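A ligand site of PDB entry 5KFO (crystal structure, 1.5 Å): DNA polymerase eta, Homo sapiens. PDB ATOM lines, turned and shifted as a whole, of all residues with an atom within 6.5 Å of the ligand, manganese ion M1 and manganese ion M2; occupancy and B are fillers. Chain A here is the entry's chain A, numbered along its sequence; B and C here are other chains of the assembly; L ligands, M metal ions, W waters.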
ATOM      1  N   ASP A  16      15.916   7.922   9.315  1.00  0.00           N
ATOM      2  CA  ASP A  16      16.097   7.067  10.494  1.00  0.00           C
ATOM      3  C   ASP A  16      16.678   7.877  11.646  1.00  0.00           C
ATOM      4  O   ASP A  16      17.733   8.482  11.495  1.00  0.00           O
ATOM      5  CB  ASP A  16      17.011   5.897  10.159  1.00  0.00           C
ATOM      6  CG  ASP A  16      17.160   4.953  11.302  1.00  0.00           C
ATOM      7  OD1 ASP A  16      17.974   5.236  12.185  1.00  0.00           O
ATOM      8  OD2 ASP A  16      16.443   3.929  11.313  1.00  0.00           O
ATOM      9  N   MET A  17      16.018   7.879  12.803  1.00  0.00           N
ATOM     10  CA  MET A  17      16.486   8.697  13.910  1.00  0.00           C
ATOM     11  C   MET A  17      17.836   8.240  14.448  1.00  0.00           C
ATOM     12  O   MET A  17      18.112   7.049  14.465  1.00  0.00           O
ATOM     13  CB  MET A  17      15.450   8.698  15.044  1.00  0.00           C
ATOM     14  CG  MET A  17      14.045   9.034  14.600  1.00  0.00           C
ATOM     15  SD  MET A  17      13.896  10.618  13.746  1.00  0.00           S
ATOM     16  CE  MET A  17      14.416  11.750  14.998  1.00  0.00           C
ATOM     17  N   ASP A  18      18.672   9.171  14.878  1.00  0.00           N
ATOM     18  CA  ASP A  18      19.972   8.794  15.467  1.00  0.00           C
ATOM     19  C   ASP A  18      19.760   8.357  16.906  1.00  0.00           C
ATOM     20  O   ASP A  18      19.023   9.021  17.633  1.00  0.00           O
ATOM     21  CB  ASP A  18      20.953   9.961  15.395  1.00  0.00           C
ATOM     22  CG  ASP A  18      21.259  10.404  13.968  1.00  0.00           C
ATOM     23  OD1 ASP A  18      21.186   9.572  13.034  1.00  0.00           O
ATOM     24  OD2 ASP A  18      21.581  11.588  13.793  1.00  0.00           O
ATOM     25  N   CYS A  19      20.392   7.239  17.262  1.00  0.00           N
ATOM     26  CA  CYS A  19      20.311   6.645  18.601  1.00  0.00           C
ATOM     27  C   CYS A  19      19.004   7.026  19.305  1.00  0.00           C
ATOM     28  O   CYS A  19      19.005   7.708  20.334  1.00  0.00           O
ATOM     29  CB  CYS A  19      21.553   7.032  19.446  1.00  0.00           C
ATOM     30  SG  CYS A  19      21.998   8.768  19.618  1.00  0.00           S
ATOM     31  N   PHE A  20      17.888   6.600  18.732  1.00  0.00           N
ATOM     32  CA  PHE A  20      16.591   7.205  19.023  1.00  0.00           C
ATOM     33  C   PHE A  20      16.186   7.225  20.499  1.00  0.00           C
ATOM     34  O   PHE A  20      15.888   8.295  21.021  1.00  0.00           O
ATOM     35  CB  PHE A  20      15.485   6.498  18.227  1.00  0.00           C
ATOM     36  CG  PHE A  20      14.144   7.165  18.349  1.00  0.00           C
ATOM     37  CD1 PHE A  20      14.058   8.552  18.275  1.00  0.00           C
ATOM     38  CD2 PHE A  20      12.985   6.428  18.534  1.00  0.00           C
ATOM     39  CE1 PHE A  20      12.812   9.202  18.386  1.00  0.00           C
ATOM     40  CE2 PHE A  20      11.727   7.072  18.647  1.00  0.00           C
ATOM     41  CZ  PHE A  20      11.660   8.450  18.570  1.00  0.00           C
ATOM     42  N   PHE A  21      16.162   6.076  21.151  1.00  0.00           N
ATOM     43  CA  PHE A  21      15.675   6.092  22.535  1.00  0.00           C
ATOM     44  C   PHE A  21      16.581   6.963  23.416  1.00  0.00           C
ATOM     45  O   PHE A  21      16.128   7.584  24.385  1.00  0.00           O
ATOM     46  CB  PHE A  21      15.593   4.680  23.141  1.00  0.00           C
ATOM     47  CG  PHE A  21      14.489   3.807  22.578  1.00  0.00           C
ATOM     48  CD1 PHE A  21      13.800   4.140  21.416  1.00  0.00           C
ATOM     49  CD2 PHE A  21      14.165   2.634  23.220  1.00  0.00           C
ATOM     50  CE1 PHE A  21      12.789   3.286  20.915  1.00  0.00           C
ATOM     51  CE2 PHE A  21      13.163   1.796  22.735  1.00  0.00           C
ATOM     52  CZ  PHE A  21      12.481   2.118  21.579  1.00  0.00           C
ATOM     53  N   VAL A  22      17.885   6.970  23.107  1.00  0.00           N
ATOM     54  CA  VAL A  22      18.810   7.834  23.844  1.00  0.00           C
ATOM     55  C   VAL A  22      18.441   9.304  23.632  1.00  0.00           C
ATOM     56  O   VAL A  22      18.394  10.066  24.597  1.00  0.00           O
ATOM     57  CB  VAL A  22      20.258   7.570  23.408  1.00  0.00           C
ATOM     58  CG1 VAL A  22      21.181   8.706  23.888  1.00  0.00           C
ATOM     59  CG2 VAL A  22      20.745   6.214  23.933  1.00  0.00           C
ATOM     60  N   GLN A  41      16.986  -1.792  29.814  1.00  0.00           N
ATOM     61  CA  GLN A  41      15.743  -2.420  30.272  1.00  0.00           C
ATOM     62  C   GLN A  41      16.063  -3.334  31.437  1.00  0.00           C
ATOM     63  O   GLN A  41      16.957  -4.170  31.328  1.00  0.00           O
ATOM     64  CB  GLN A  41      15.093  -3.243  29.162  1.00  0.00           C
ATOM     65  CG  GLN A  41      14.047  -2.537  28.359  1.00  0.00           C
ATOM     66  CD  GLN A  41      13.599  -3.341  27.154  1.00  0.00           C
ATOM     67  OE1 GLN A  41      14.253  -4.299  26.742  1.00  0.00           O
ATOM     68  NE2 GLN A  41      12.462  -2.964  26.591  1.00  0.00           N
ATOM     69  N   ILE A  51      19.582  -1.256  25.106  1.00  0.00           N
ATOM     70  CA  ILE A  51      18.853  -1.313  23.843  1.00  0.00           C
ATOM     71  C   ILE A  51      19.123  -0.117  22.925  1.00  0.00           C
ATOM     72  O   ILE A  51      18.739  -0.138  21.754  1.00  0.00           O
ATOM     73  CB  ILE A  51      17.328  -1.453  24.076  1.00  0.00           C
ATOM     74  CG1 ILE A  51      16.768  -0.280  24.892  1.00  0.00           C
ATOM     75  CG2 ILE A  51      17.022  -2.800  24.737  1.00  0.00           C
ATOM     76  CD1 ILE A  51      15.225  -0.314  24.971  1.00  0.00           C
ATOM     77  N   ALA A  52      19.801   0.909  23.428  1.00  0.00           N
ATOM     78  CA  ALA A  52      20.186   2.055  22.591  1.00  0.00           C
ATOM     79  C   ALA A  52      21.432   2.704  23.186  1.00  0.00           C
ATOM     80  O   ALA A  52      21.602   2.704  24.416  1.00  0.00           O
ATOM     81  CB  ALA A  52      19.039   3.083  22.471  1.00  0.00           C
ATOM     82  N   VAL A  53      22.294   3.242  22.313  1.00  0.00           N
ATOM     83  CA  VAL A  53      23.628   3.697  22.707  1.00  0.00           C
ATOM     84  C   VAL A  53      23.977   5.016  22.022  1.00  0.00           C
ATOM     85  O   VAL A  53      23.919   5.091  20.790  1.00  0.00           O
ATOM     86  CB  VAL A  53      24.722   2.648  22.321  1.00  0.00           C
ATOM     87  CG1 VAL A  53      26.078   3.028  22.911  1.00  0.00           C
ATOM     88  CG2 VAL A  53      24.330   1.271  22.812  1.00  0.00           C
ATOM     89  N   TYR A  55      26.350   8.016  20.479  1.00  0.00           N
ATOM     90  CA  TYR A  55      27.549   7.871  19.672  1.00  0.00           C
ATOM     91  C   TYR A  55      28.818   8.055  20.486  1.00  0.00           C
ATOM     92  O   TYR A  55      29.820   7.388  20.207  1.00  0.00           O
ATOM     93  CB  TYR A  55      27.506   8.823  18.460  1.00  0.00           C
ATOM     94  CG  TYR A  55      26.637   8.238  17.379  1.00  0.00           C
ATOM     95  CD1 TYR A  55      25.253   8.328  17.447  1.00  0.00           C
ATOM     96  CD2 TYR A  55      27.189   7.499  16.341  1.00  0.00           C
ATOM     97  CE1 TYR A  55      24.443   7.756  16.507  1.00  0.00           C
ATOM     98  CE2 TYR A  55      26.383   6.913  15.375  1.00  0.00           C
ATOM     99  CZ  TYR A  55      25.014   7.040  15.459  1.00  0.00           C
ATOM    100  OH  TYR A  55      24.205   6.464  14.510  1.00  0.00           O
ATOM    101  N   ARG A  58      29.322   4.643  21.911  1.00  0.00           N
ATOM    102  CA  ARG A  58      29.786   3.690  20.899  1.00  0.00           C
ATOM    103  C   ARG A  58      31.298   3.750  20.685  1.00  0.00           C
ATOM    104  O   ARG A  58      31.924   2.729  20.361  1.00  0.00           O
ATOM    105  CB  ARG A  58      29.079   3.923  19.569  1.00  0.00           C
ATOM    106  CG  ARG A  58      27.592   3.802  19.682  1.00  0.00           C
ATOM    107  CD  ARG A  58      26.912   3.946  18.337  1.00  0.00           C
ATOM    108  NE  ARG A  58      25.470   4.122  18.533  1.00  0.00           N
ATOM    109  CZ  ARG A  58      24.558   4.064  17.578  1.00  0.00           C
ATOM    110  NH1 ARG A  58      24.921   3.805  16.322  1.00  0.00           N
ATOM    111  NH2 ARG A  58      23.266   4.256  17.893  1.00  0.00           N
ATOM    112  N   ARG A  64      24.312  -2.309  21.566  1.00  0.00           N
ATOM    113  CA  ARG A  64      23.059  -2.971  21.879  1.00  0.00           C
ATOM    114  C   ARG A  64      23.309  -4.433  22.253  1.00  0.00           C
ATOM    115  O   ARG A  64      24.256  -5.041  21.770  1.00  0.00           O
ATOM    116  CB  ARG A  64      22.109  -2.840  20.685  1.00  0.00           C
ATOM    117  CG  ARG A  64      20.851  -3.654  20.783  1.00  0.00           C
ATOM    118  CD  ARG A  64      19.946  -3.355  19.605  1.00  0.00           C
ATOM    119  NE  ARG A  64      19.629  -1.943  19.573  1.00  0.00           N
ATOM    120  CZ  ARG A  64      19.924  -1.119  18.567  1.00  0.00           C
ATOM    121  NH1 ARG A  64      20.523  -1.585  17.476  1.00  0.00           N
ATOM    122  NH2 ARG A  64      19.581   0.155  18.666  1.00  0.00           N
ATOM    123  N   LEU A  92       7.120   0.710  26.655  1.00  0.00           N
ATOM    124  CA  LEU A  92       7.793   1.540  25.636  1.00  0.00           C
ATOM    125  C   LEU A  92       6.984   2.749  25.189  1.00  0.00           C
ATOM    126  O   LEU A  92       7.310   3.364  24.166  1.00  0.00           O
ATOM    127  CB  LEU A  92       8.143   0.669  24.420  1.00  0.00           C
ATOM    128  CG  LEU A  92       8.947  -0.598  24.725  1.00  0.00           C
ATOM    129  CD1 LEU A  92       9.151  -1.431  23.453  1.00  0.00           C
ATOM    130  CD2 LEU A  92      10.289  -0.197  25.346  1.00  0.00           C
ATOM    131  N   SER A 116       9.632   1.247  11.160  1.00  0.00           N
ATOM    132  CA  SER A 116       9.979   0.835  12.522  1.00  0.00           C
ATOM    133  C   SER A 116       9.556   1.944  13.476  1.00  0.00           C
ATOM    134  O   SER A 116       9.025   2.957  13.056  1.00  0.00           O
ATOM    135  CB  SER A 116      11.470   0.572  12.683  1.00  0.00           C
ATOM    136  OG  SER A 116      12.183   1.808  12.784  1.00  0.00           O
ATOM    137  N   ILE A 117       9.865   1.779  14.763  1.00  0.00           N
ATOM    138  CA  ILE A 117       9.540   2.834  15.705  1.00  0.00           C
ATOM    139  C   ILE A 117      10.326   4.125  15.406  1.00  0.00           C
ATOM    140  O   ILE A 117       9.926   5.209  15.811  1.00  0.00           O
ATOM    141  CB  ILE A 117       9.807   2.367  17.155  1.00  0.00           C
ATOM    142  CG1 ILE A 117       9.076   3.261  18.159  1.00  0.00           C
ATOM    143  CG2 ILE A 117      11.300   2.323  17.448  1.00  0.00           C
ATOM    144  CD1 ILE A 117       9.067   2.668  19.578  1.00  0.00           C
ATOM    145  N   ASP A 118      11.445   4.016  14.681  1.00  0.00           N
ATOM    146  CA  ASP A 118      12.264   5.220  14.493  1.00  0.00           C
ATOM    147  C   ASP A 118      12.607   5.531  13.019  1.00  0.00           C
ATOM    148  O   ASP A 118      13.516   6.335  12.756  1.00  0.00           O
ATOM    149  CB  ASP A 118      13.566   5.135  15.312  1.00  0.00           C
ATOM    150  CG  ASP A 118      14.723   4.527  14.538  1.00  0.00           C
ATOM    151  OD1 ASP A 118      14.555   3.519  13.793  1.00  0.00           O
ATOM    152  OD2 ASP A 118      15.808   5.146  14.627  1.00  0.00           O
ATOM    153  N   GLU A 119      11.892   4.943  12.068  1.00  0.00           N
ATOM    154  CA  GLU A 119      12.183   5.265  10.671  1.00  0.00           C
ATOM    155  C   GLU A 119      11.011   5.101   9.758  1.00  0.00           C
ATOM    156  O   GLU A 119      10.092   4.304  10.026  1.00  0.00           O
ATOM    157  CB  GLU A 119      13.344   4.425  10.144  1.00  0.00           C
ATOM    158  CG  GLU A 119      12.987   2.976   9.859  1.00  0.00           C
ATOM    159  CD  GLU A 119      14.184   2.069  10.046  1.00  0.00           C
ATOM    160  OE1 GLU A 119      14.841   1.733   9.042  1.00  0.00           O
ATOM    161  OE2 GLU A 119      14.476   1.717  11.204  1.00  0.00           O
ATOM    162  N   SER A 216      19.324  10.772  10.449  1.00  0.00           N
ATOM    163  CA  SER A 216      20.043  10.629   9.195  1.00  0.00           C
ATOM    164  C   SER A 216      19.065  10.229   8.120  1.00  0.00           C
ATOM    165  O   SER A 216      17.924   9.896   8.418  1.00  0.00           O
ATOM    166  CB  SER A 216      21.146   9.584   9.341  1.00  0.00           C
ATOM    167  OG  SER A 216      22.069  10.005  10.325  1.00  0.00           O
ATOM    168  N   LYS A 227      17.635   2.882   2.227  1.00  0.00           N
ATOM    169  CA  LYS A 227      18.018   2.370   3.535  1.00  0.00           C
ATOM    170  C   LYS A 227      19.534   2.203   3.647  1.00  0.00           C
ATOM    171  O   LYS A 227      20.158   2.592   4.648  1.00  0.00           O
ATOM    172  CB  LYS A 227      17.310   1.030   3.817  1.00  0.00           C
ATOM    173  CG  LYS A 227      17.720   0.374   5.140  1.00  0.00           C
ATOM    174  CD  LYS A 227      17.373   1.226   6.367  1.00  0.00           C
ATOM    175  CE  LYS A 227      17.716   0.453   7.641  1.00  0.00           C
ATOM    176  NZ  LYS A 227      17.504   1.237   8.904  1.00  0.00           N
ATOM    177  N   LYS A 234      25.863   8.222   8.957  1.00  0.00           N
ATOM    178  CA  LYS A 234      25.358   8.486  10.304  1.00  0.00           C
ATOM    179  C   LYS A 234      26.454   8.910  11.280  1.00  0.00           C
ATOM    180  O   LYS A 234      27.576   8.430  11.181  1.00  0.00           O
ATOM    181  CB  LYS A 234      24.664   7.237  10.873  1.00  0.00           C
ATOM    182  CG  LYS A 234      23.221   7.045  10.477  1.00  0.00           C
ATOM    183  CD  LYS A 234      22.517   6.008  11.365  1.00  0.00           C
ATOM    184  CE  LYS A 234      20.982   6.083  11.244  1.00  0.00           C
ATOM    185  NZ  LYS A 234      20.355   6.945  12.306  1.00  0.00           N
ATOM    186  N   PRO A 235      26.129   9.795  12.237  1.00  0.00           N
ATOM    187  CA  PRO A 235      24.822  10.394  12.483  1.00  0.00           C
ATOM    188  C   PRO A 235      24.695  11.806  11.937  1.00  0.00           C
ATOM    189  O   PRO A 235      25.680  12.419  11.516  1.00  0.00           O
ATOM    190  CB  PRO A 235      24.756  10.433  14.013  1.00  0.00           C
ATOM    191  CG  PRO A 235      26.186  10.775  14.393  1.00  0.00           C
ATOM    192  CD  PRO A 235      27.071  10.111  13.330  1.00  0.00           C
ATOM    193  P    DT B   8      15.440  -2.728   8.919  1.00  0.00           P
ATOM    194  OP1  DT B   8      14.726  -2.041   7.831  1.00  0.00           O
ATOM    195  OP2  DT B   8      16.897  -2.936   8.835  1.00  0.00           O
ATOM    196  O5'  DT B   8      15.082  -1.874  10.189  1.00  0.00           O
ATOM    197  C5'  DT B   8      15.534  -2.286  11.370  1.00  0.00           C
ATOM    198  C4'  DT B   8      14.769  -1.646  12.476  1.00  0.00           C
ATOM    199  O4'  DT B   8      14.197  -2.721  13.245  1.00  0.00           O
ATOM    200  C3'  DT B   8      15.703  -0.882  13.398  1.00  0.00           C
ATOM    201  O3'  DT B   8      15.191   0.407  13.729  1.00  0.00           O
ATOM    202  C2'  DT B   8      15.870  -1.793  14.618  1.00  0.00           C
ATOM    203  C1'  DT B   8      14.599  -2.628  14.598  1.00  0.00           C
ATOM    204  N1   DT B   8      14.815  -4.001  15.124  1.00  0.00           N
ATOM    205  C2   DT B   8      14.090  -4.406  16.221  1.00  0.00           C
ATOM    206  O2   DT B   8      13.290  -3.676  16.775  1.00  0.00           O
ATOM    207  N3   DT B   8      14.338  -5.680  16.640  1.00  0.00           N
ATOM    208  C4   DT B   8      15.224  -6.576  16.101  1.00  0.00           C
ATOM    209  O4   DT B   8      15.384  -7.711  16.566  1.00  0.00           O
ATOM    210  C5   DT B   8      15.957  -6.104  14.955  1.00  0.00           C
ATOM    211  C7   DT B   8      16.953  -7.015  14.280  1.00  0.00           C
ATOM    212  C6   DT B   8      15.719  -4.854  14.518  1.00  0.00           C
ATOM    213  P    DT C   3      21.943 -14.340  27.064  1.00  0.00           P
ATOM    214  OP1  DT C   3      21.695 -15.684  26.483  1.00  0.00           O
ATOM    215  OP2  DT C   3      23.320 -13.931  27.421  1.00  0.00           O
ATOM    216  O5'  DT C   3      21.339 -13.248  26.067  1.00  0.00           O
ATOM    217  C5'  DT C   3      21.234 -11.891  26.482  1.00  0.00           C
ATOM    218  C4'  DT C   3      20.399 -11.100  25.490  1.00  0.00           C
ATOM    219  O4'  DT C   3      21.178 -10.858  24.296  1.00  0.00           O
ATOM    220  C3'  DT C   3      19.131 -11.813  25.032  1.00  0.00           C
ATOM    221  O3'  DT C   3      17.971 -11.106  25.484  1.00  0.00           O
ATOM    222  C2'  DT C   3      19.217 -11.861  23.498  1.00  0.00           C
ATOM    223  C1'  DT C   3      20.350 -10.901  23.172  1.00  0.00           C
ATOM    224  N1   DT C   3      21.158 -11.345  21.997  1.00  0.00           N
ATOM    225  C2   DT C   3      21.202 -10.560  20.869  1.00  0.00           C
ATOM    226  O2   DT C   3      20.611  -9.507  20.765  1.00  0.00           O
ATOM    227  N3   DT C   3      21.982 -11.062  19.862  1.00  0.00           N
ATOM    228  C4   DT C   3      22.699 -12.248  19.864  1.00  0.00           C
ATOM    229  O4   DT C   3      23.369 -12.616  18.902  1.00  0.00           O
ATOM    230  C5   DT C   3      22.612 -13.019  21.081  1.00  0.00           C
ATOM    231  C7   DT C   3      23.344 -14.315  21.206  1.00  0.00           C
ATOM    232  C6   DT C   3      21.851 -12.540  22.082  1.00  0.00           C
ATOM    233  P    DT C   4      16.116 -12.375  27.756  1.00  0.00           P
ATOM    234  OP1  DT C   4      15.883 -12.513  29.209  1.00  0.00           O
ATOM    235  OP2  DT C   4      15.733 -13.448  26.817  1.00  0.00           O
ATOM    236  O5'  DT C   4      15.362 -11.063  27.273  1.00  0.00           O
ATOM    237  C5'  DT C   4      15.706  -9.833  27.840  1.00  0.00           C
ATOM    238  C4'  DT C   4      14.722  -8.763  27.409  1.00  0.00           C
ATOM    239  O4'  DT C   4      15.142  -8.131  26.184  1.00  0.00           O
ATOM    240  C3'  DT C   4      13.291  -9.206  27.179  1.00  0.00           C
ATOM    241  O3'  DT C   4      12.422  -8.222  27.694  1.00  0.00           O
ATOM    242  C2'  DT C   4      13.198  -9.296  25.641  1.00  0.00           C
ATOM    243  C1'  DT C   4      14.075  -8.126  25.261  1.00  0.00           C
ATOM    244  N1   DT C   4      14.686  -8.185  23.932  1.00  0.00           N
ATOM    245  C2   DT C   4      14.808  -6.998  23.262  1.00  0.00           C
ATOM    246  O2   DT C   4      14.360  -5.954  23.694  1.00  0.00           O
ATOM    247  N3   DT C   4      15.448  -7.096  22.063  1.00  0.00           N
ATOM    248  C4   DT C   4      15.986  -8.215  21.479  1.00  0.00           C
ATOM    249  O4   DT C   4      16.533  -8.168  20.382  1.00  0.00           O
ATOM    250  C5   DT C   4      15.859  -9.429  22.256  1.00  0.00           C
ATOM    251  C7   DT C   4      16.403 -10.738  21.721  1.00  0.00           C
ATOM    252  C6   DT C   4      15.228  -9.351  23.444  1.00  0.00           C
ATOM    253  P    DA C   5      10.834  -8.383  27.605  1.00  0.00           P
ATOM    254  OP1  DA C   5      10.259  -7.846  28.857  1.00  0.00           O
ATOM    255  OP2  DA C   5      10.515  -9.748  27.141  1.00  0.00           O
ATOM    256  O5'  DA C   5      10.425  -7.425  26.414  1.00  0.00           O
ATOM    257  C5'  DA C   5      10.567  -6.009  26.567  1.00  0.00           C
ATOM    258  C4'  DA C   5       9.985  -5.315  25.358  1.00  0.00           C
ATOM    259  O4'  DA C   5      10.845  -5.555  24.204  1.00  0.00           O
ATOM    260  C3'  DA C   5       8.587  -5.788  24.952  1.00  0.00           C
ATOM    261  O3'  DA C   5       7.817  -4.670  24.517  1.00  0.00           O
ATOM    262  C2'  DA C   5       8.868  -6.744  23.797  1.00  0.00           C
ATOM    263  C1'  DA C   5      10.056  -6.039  23.148  1.00  0.00           C
ATOM    264  N9   DA C   5      10.893  -6.895  22.324  1.00  0.00           N
ATOM    265  C8   DA C   5      11.201  -8.209  22.543  1.00  0.00           C
ATOM    266  N7   DA C   5      11.999  -8.721  21.647  1.00  0.00           N
ATOM    267  C5   DA C   5      12.235  -7.669  20.770  1.00  0.00           C
ATOM    268  C6   DA C   5      12.999  -7.566  19.594  1.00  0.00           C
ATOM    269  N6   DA C   5      13.701  -8.580  19.081  1.00  0.00           N
ATOM    270  N1   DA C   5      13.024  -6.380  18.967  1.00  0.00           N
ATOM    271  C2   DA C   5      12.311  -5.358  19.486  1.00  0.00           C
ATOM    272  N3   DA C   5      11.559  -5.330  20.579  1.00  0.00           N
ATOM    273  C4   DA C   5      11.567  -6.542  21.179  1.00  0.00           C
HETATM  274  P1  LIG L   1      21.251   4.529  14.947  1.00  0.00           P
HETATM  275  O1  LIG L   1      20.074   4.444  14.116  1.00  0.00           O
HETATM  276  O2  LIG L   1      21.672   5.914  15.035  1.00  0.00           O
HETATM  277  O3  LIG L   1      22.366   3.593  14.617  1.00  0.00           O
HETATM  278  P2  LIG L   1      19.328   3.718  16.929  1.00  0.00           P
HETATM  279  O4  LIG L   1      18.301   4.692  16.534  1.00  0.00           O
HETATM  280  O5  LIG L   1      19.309   3.553  18.396  1.00  0.00           O
HETATM  281  O6  LIG L   1      20.772   4.171  16.415  1.00  0.00           O
HETATM  282  P3  LIG L   1      17.982   1.689  15.391  1.00  0.00           P
HETATM  283  S1  LIG L   1      18.758   0.002  14.747  1.00  0.00           S
HETATM  284  O7  LIG L   1      17.496   2.558  14.319  1.00  0.00           O
HETATM  285  O8  LIG L   1      19.165   2.282  16.274  1.00  0.00           O
HETATM  286  O9  LIG L   1      16.830   1.382  16.344  1.00  0.00           O
HETATM  287  C1  LIG L   1      15.945   2.343  16.708  1.00  0.00           C
HETATM  288  C2  LIG L   1      15.457   2.203  18.156  1.00  0.00           C
HETATM  289  O10 LIG L   1      14.789   0.992  18.256  1.00  0.00           O
HETATM  290  C3  LIG L   1      16.521   2.106  19.129  1.00  0.00           C
HETATM  291  O11 LIG L   1      16.901   3.342  19.687  1.00  0.00           O
HETATM  292  C4  LIG L   1      16.001   1.251  20.187  1.00  0.00           C
HETATM  293  C5  LIG L   1      15.144   0.299  19.441  1.00  0.00           C
HETATM  294  N1  LIG L   1      15.713  -0.975  19.111  1.00  0.00           N
HETATM  295  C6  LIG L   1      16.472  -1.289  18.064  1.00  0.00           C
HETATM  296  N2  LIG L   1      16.792  -2.541  18.064  1.00  0.00           N
HETATM  297  C7  LIG L   1      16.281  -3.118  19.094  1.00  0.00           C
HETATM  298  C8  LIG L   1      16.233  -4.413  19.674  1.00  0.00           C
HETATM  299  N3  LIG L   1      16.908  -5.439  19.025  1.00  0.00           N
HETATM  300  N4  LIG L   1      15.548  -4.635  20.814  1.00  0.00           N
HETATM  301  C9  LIG L   1      14.877  -3.674  21.477  1.00  0.00           C
HETATM  302  N5  LIG L   1      14.890  -2.426  20.942  1.00  0.00           N
HETATM  303  C10 LIG L   1      15.573  -2.121  19.801  1.00  0.00           C
HETATM  304 MN    MN M   1      15.977   2.312  12.656  1.00  0.00          MN
HETATM  305 MN    MN M   2      17.885   4.909  14.287  1.00  0.00          MN
HETATM  306  O   HOH W   1      22.443   0.920  15.596  1.00  0.00           O
HETATM  307  O   HOH W   2      12.542  -1.472  22.249  1.00  0.00           O
HETATM  308  O   HOH W   3      21.571   2.664  19.642  1.00  0.00           O
HETATM  309  O   HOH W   4      12.377  -1.527  18.192  1.00  0.00           O
HETATM  310  O   HOH W   5      18.456  -4.167  16.413  1.00  0.00           O
HETATM  311  O   HOH W   6      20.124   2.670  11.844  1.00  0.00           O
HETATM  312  O   HOH W   7      13.664   0.267  15.721  1.00  0.00           O
HETATM  313  O   HOH W   8      17.749   1.280  11.847  1.00  0.00           O
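The backbone NH of Asp 118 is in hydrogen-bond range of the side-chain hydroxyl of Ser 116. OD2 of Asp 16 lies close to NZ of Lys 227 (3.8 Å). The side-chain amino group of Lys 234 sits close to the backbone carbonyl oxygen of Met 17. N of Glu 119 is in hydrogen-bond range of OG of Ser 116 (3.2 Å). The guanidinium group (NH1) of Arg 58 sits at hydrogen-bond distance from the side-chain hydroxyl (OH) of Tyr 55, at 3.3 Å. NE of Arg 58 sits at hydrogen-bond distance from O of Val 53 (2.9 Å). The guanidinium group (NE) of Arg 64 is in hydrogen-bond range of the backbone carbonyl oxygen (O) of Ile 51, 3.0 Å away. OD1 of Asp 18 lies within hydrogen-bond range of OG of Ser 216 (2.9 Å).
Ser 116 touches manganese ion M1. Of the 27 residues printed, 5 come within 4 Å of manganese ion M1.
Asp 18 touches the ligand. Ile 51 touches the ligand (O to C4, 3.4 Å). CB of Ala 52 touches O11 of the ligand, 3.5 Å away. Ile 117 touches the ligand. C2 of DA 5 of chain C touches N4 of the ligand, at 3.6 Å. Hydrophobic or aromatic side chains that line the ligand: Phe 20, Phe 21, Ile 51, Ala 52, Tyr 55 and Ile 117. 17 residues have an atom within 4 Å of the ligand: Asp 16, Met 17, Asp 18, Cys 19, Phe 20, Phe 21, Ile 51, Ala 52, Tyr 55, Arg 58, Arg 64, Ile 117, Asp 118, Lys 234, DT 8 of chain B, DT 4 of chain C and DA 5 of chain C.
Manganese ion M1 is bound by OD2 of Asp 16, OE2 of Glu 119, OD1 of Asp 118, water W8, O7 of the ligand and O3' of DT 8 of chain B. Manganese ion M1 has six donor atoms within binding distance.
NZ of Lys 234 touches manganese ion M2, 3.8 Å away. The nearest printed residue that does not touch manganese ion M2 is Asp 18 (4.4 Å).
The side-chain hydroxyl (OH) of Tyr 55 sits at hydrogen-bond distance from an oxygen (O2) of the ligand (2.6 Å). O4 of DT 4 of chain C is in hydrogen-bond range of a nitrogen (N3) of the ligand, at 3.1 Å. An oxygen (O2) of the ligand is in hydrogen-bond range of the backbone NH (N) of Cys 19, at 2.9 Å. NH1 of Arg 58 lies within salt-bridge range of O3 of the ligand. The backbone NH (N) of Phe 20 sits at hydrogen-bond distance from an oxygen (O5) of the ligand (3.4 Å). NZ of Lys 234 is in salt-bridge range of O2 of the ligand (3.2 Å). The backbone NH (N) of Phe 21 lies within hydrogen-bond range of an oxygen (O11) of the ligand, 3.2 Å away. NH2 of Arg 64 lies within salt-bridge range of O5 of the ligand (3.4 Å).
Water W8 lies within hydrogen-bond range of NZ of Lys 227 and S1 of the ligand. Water W5 lies within hydrogen-bond range of N2 of the ligand (2.9 Å) and NH1 of Arg 64 (3.5 Å). Water W4 lies within hydrogen-bond range of O2 of DT 8 of chain B and O10 of the ligand.
Manganese ion M2 is bound by OD2 of Asp 118 (2.1 Å), OD1 of Asp 16 (2.1 Å), O of Met 17 (2.2 Å), O1 of the ligand (2.2 Å), O4 of the ligand (2.3 Å) and O7 of the ligand (2.4 Å). Manganese ion M2 has six donor atoms within binding distance.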
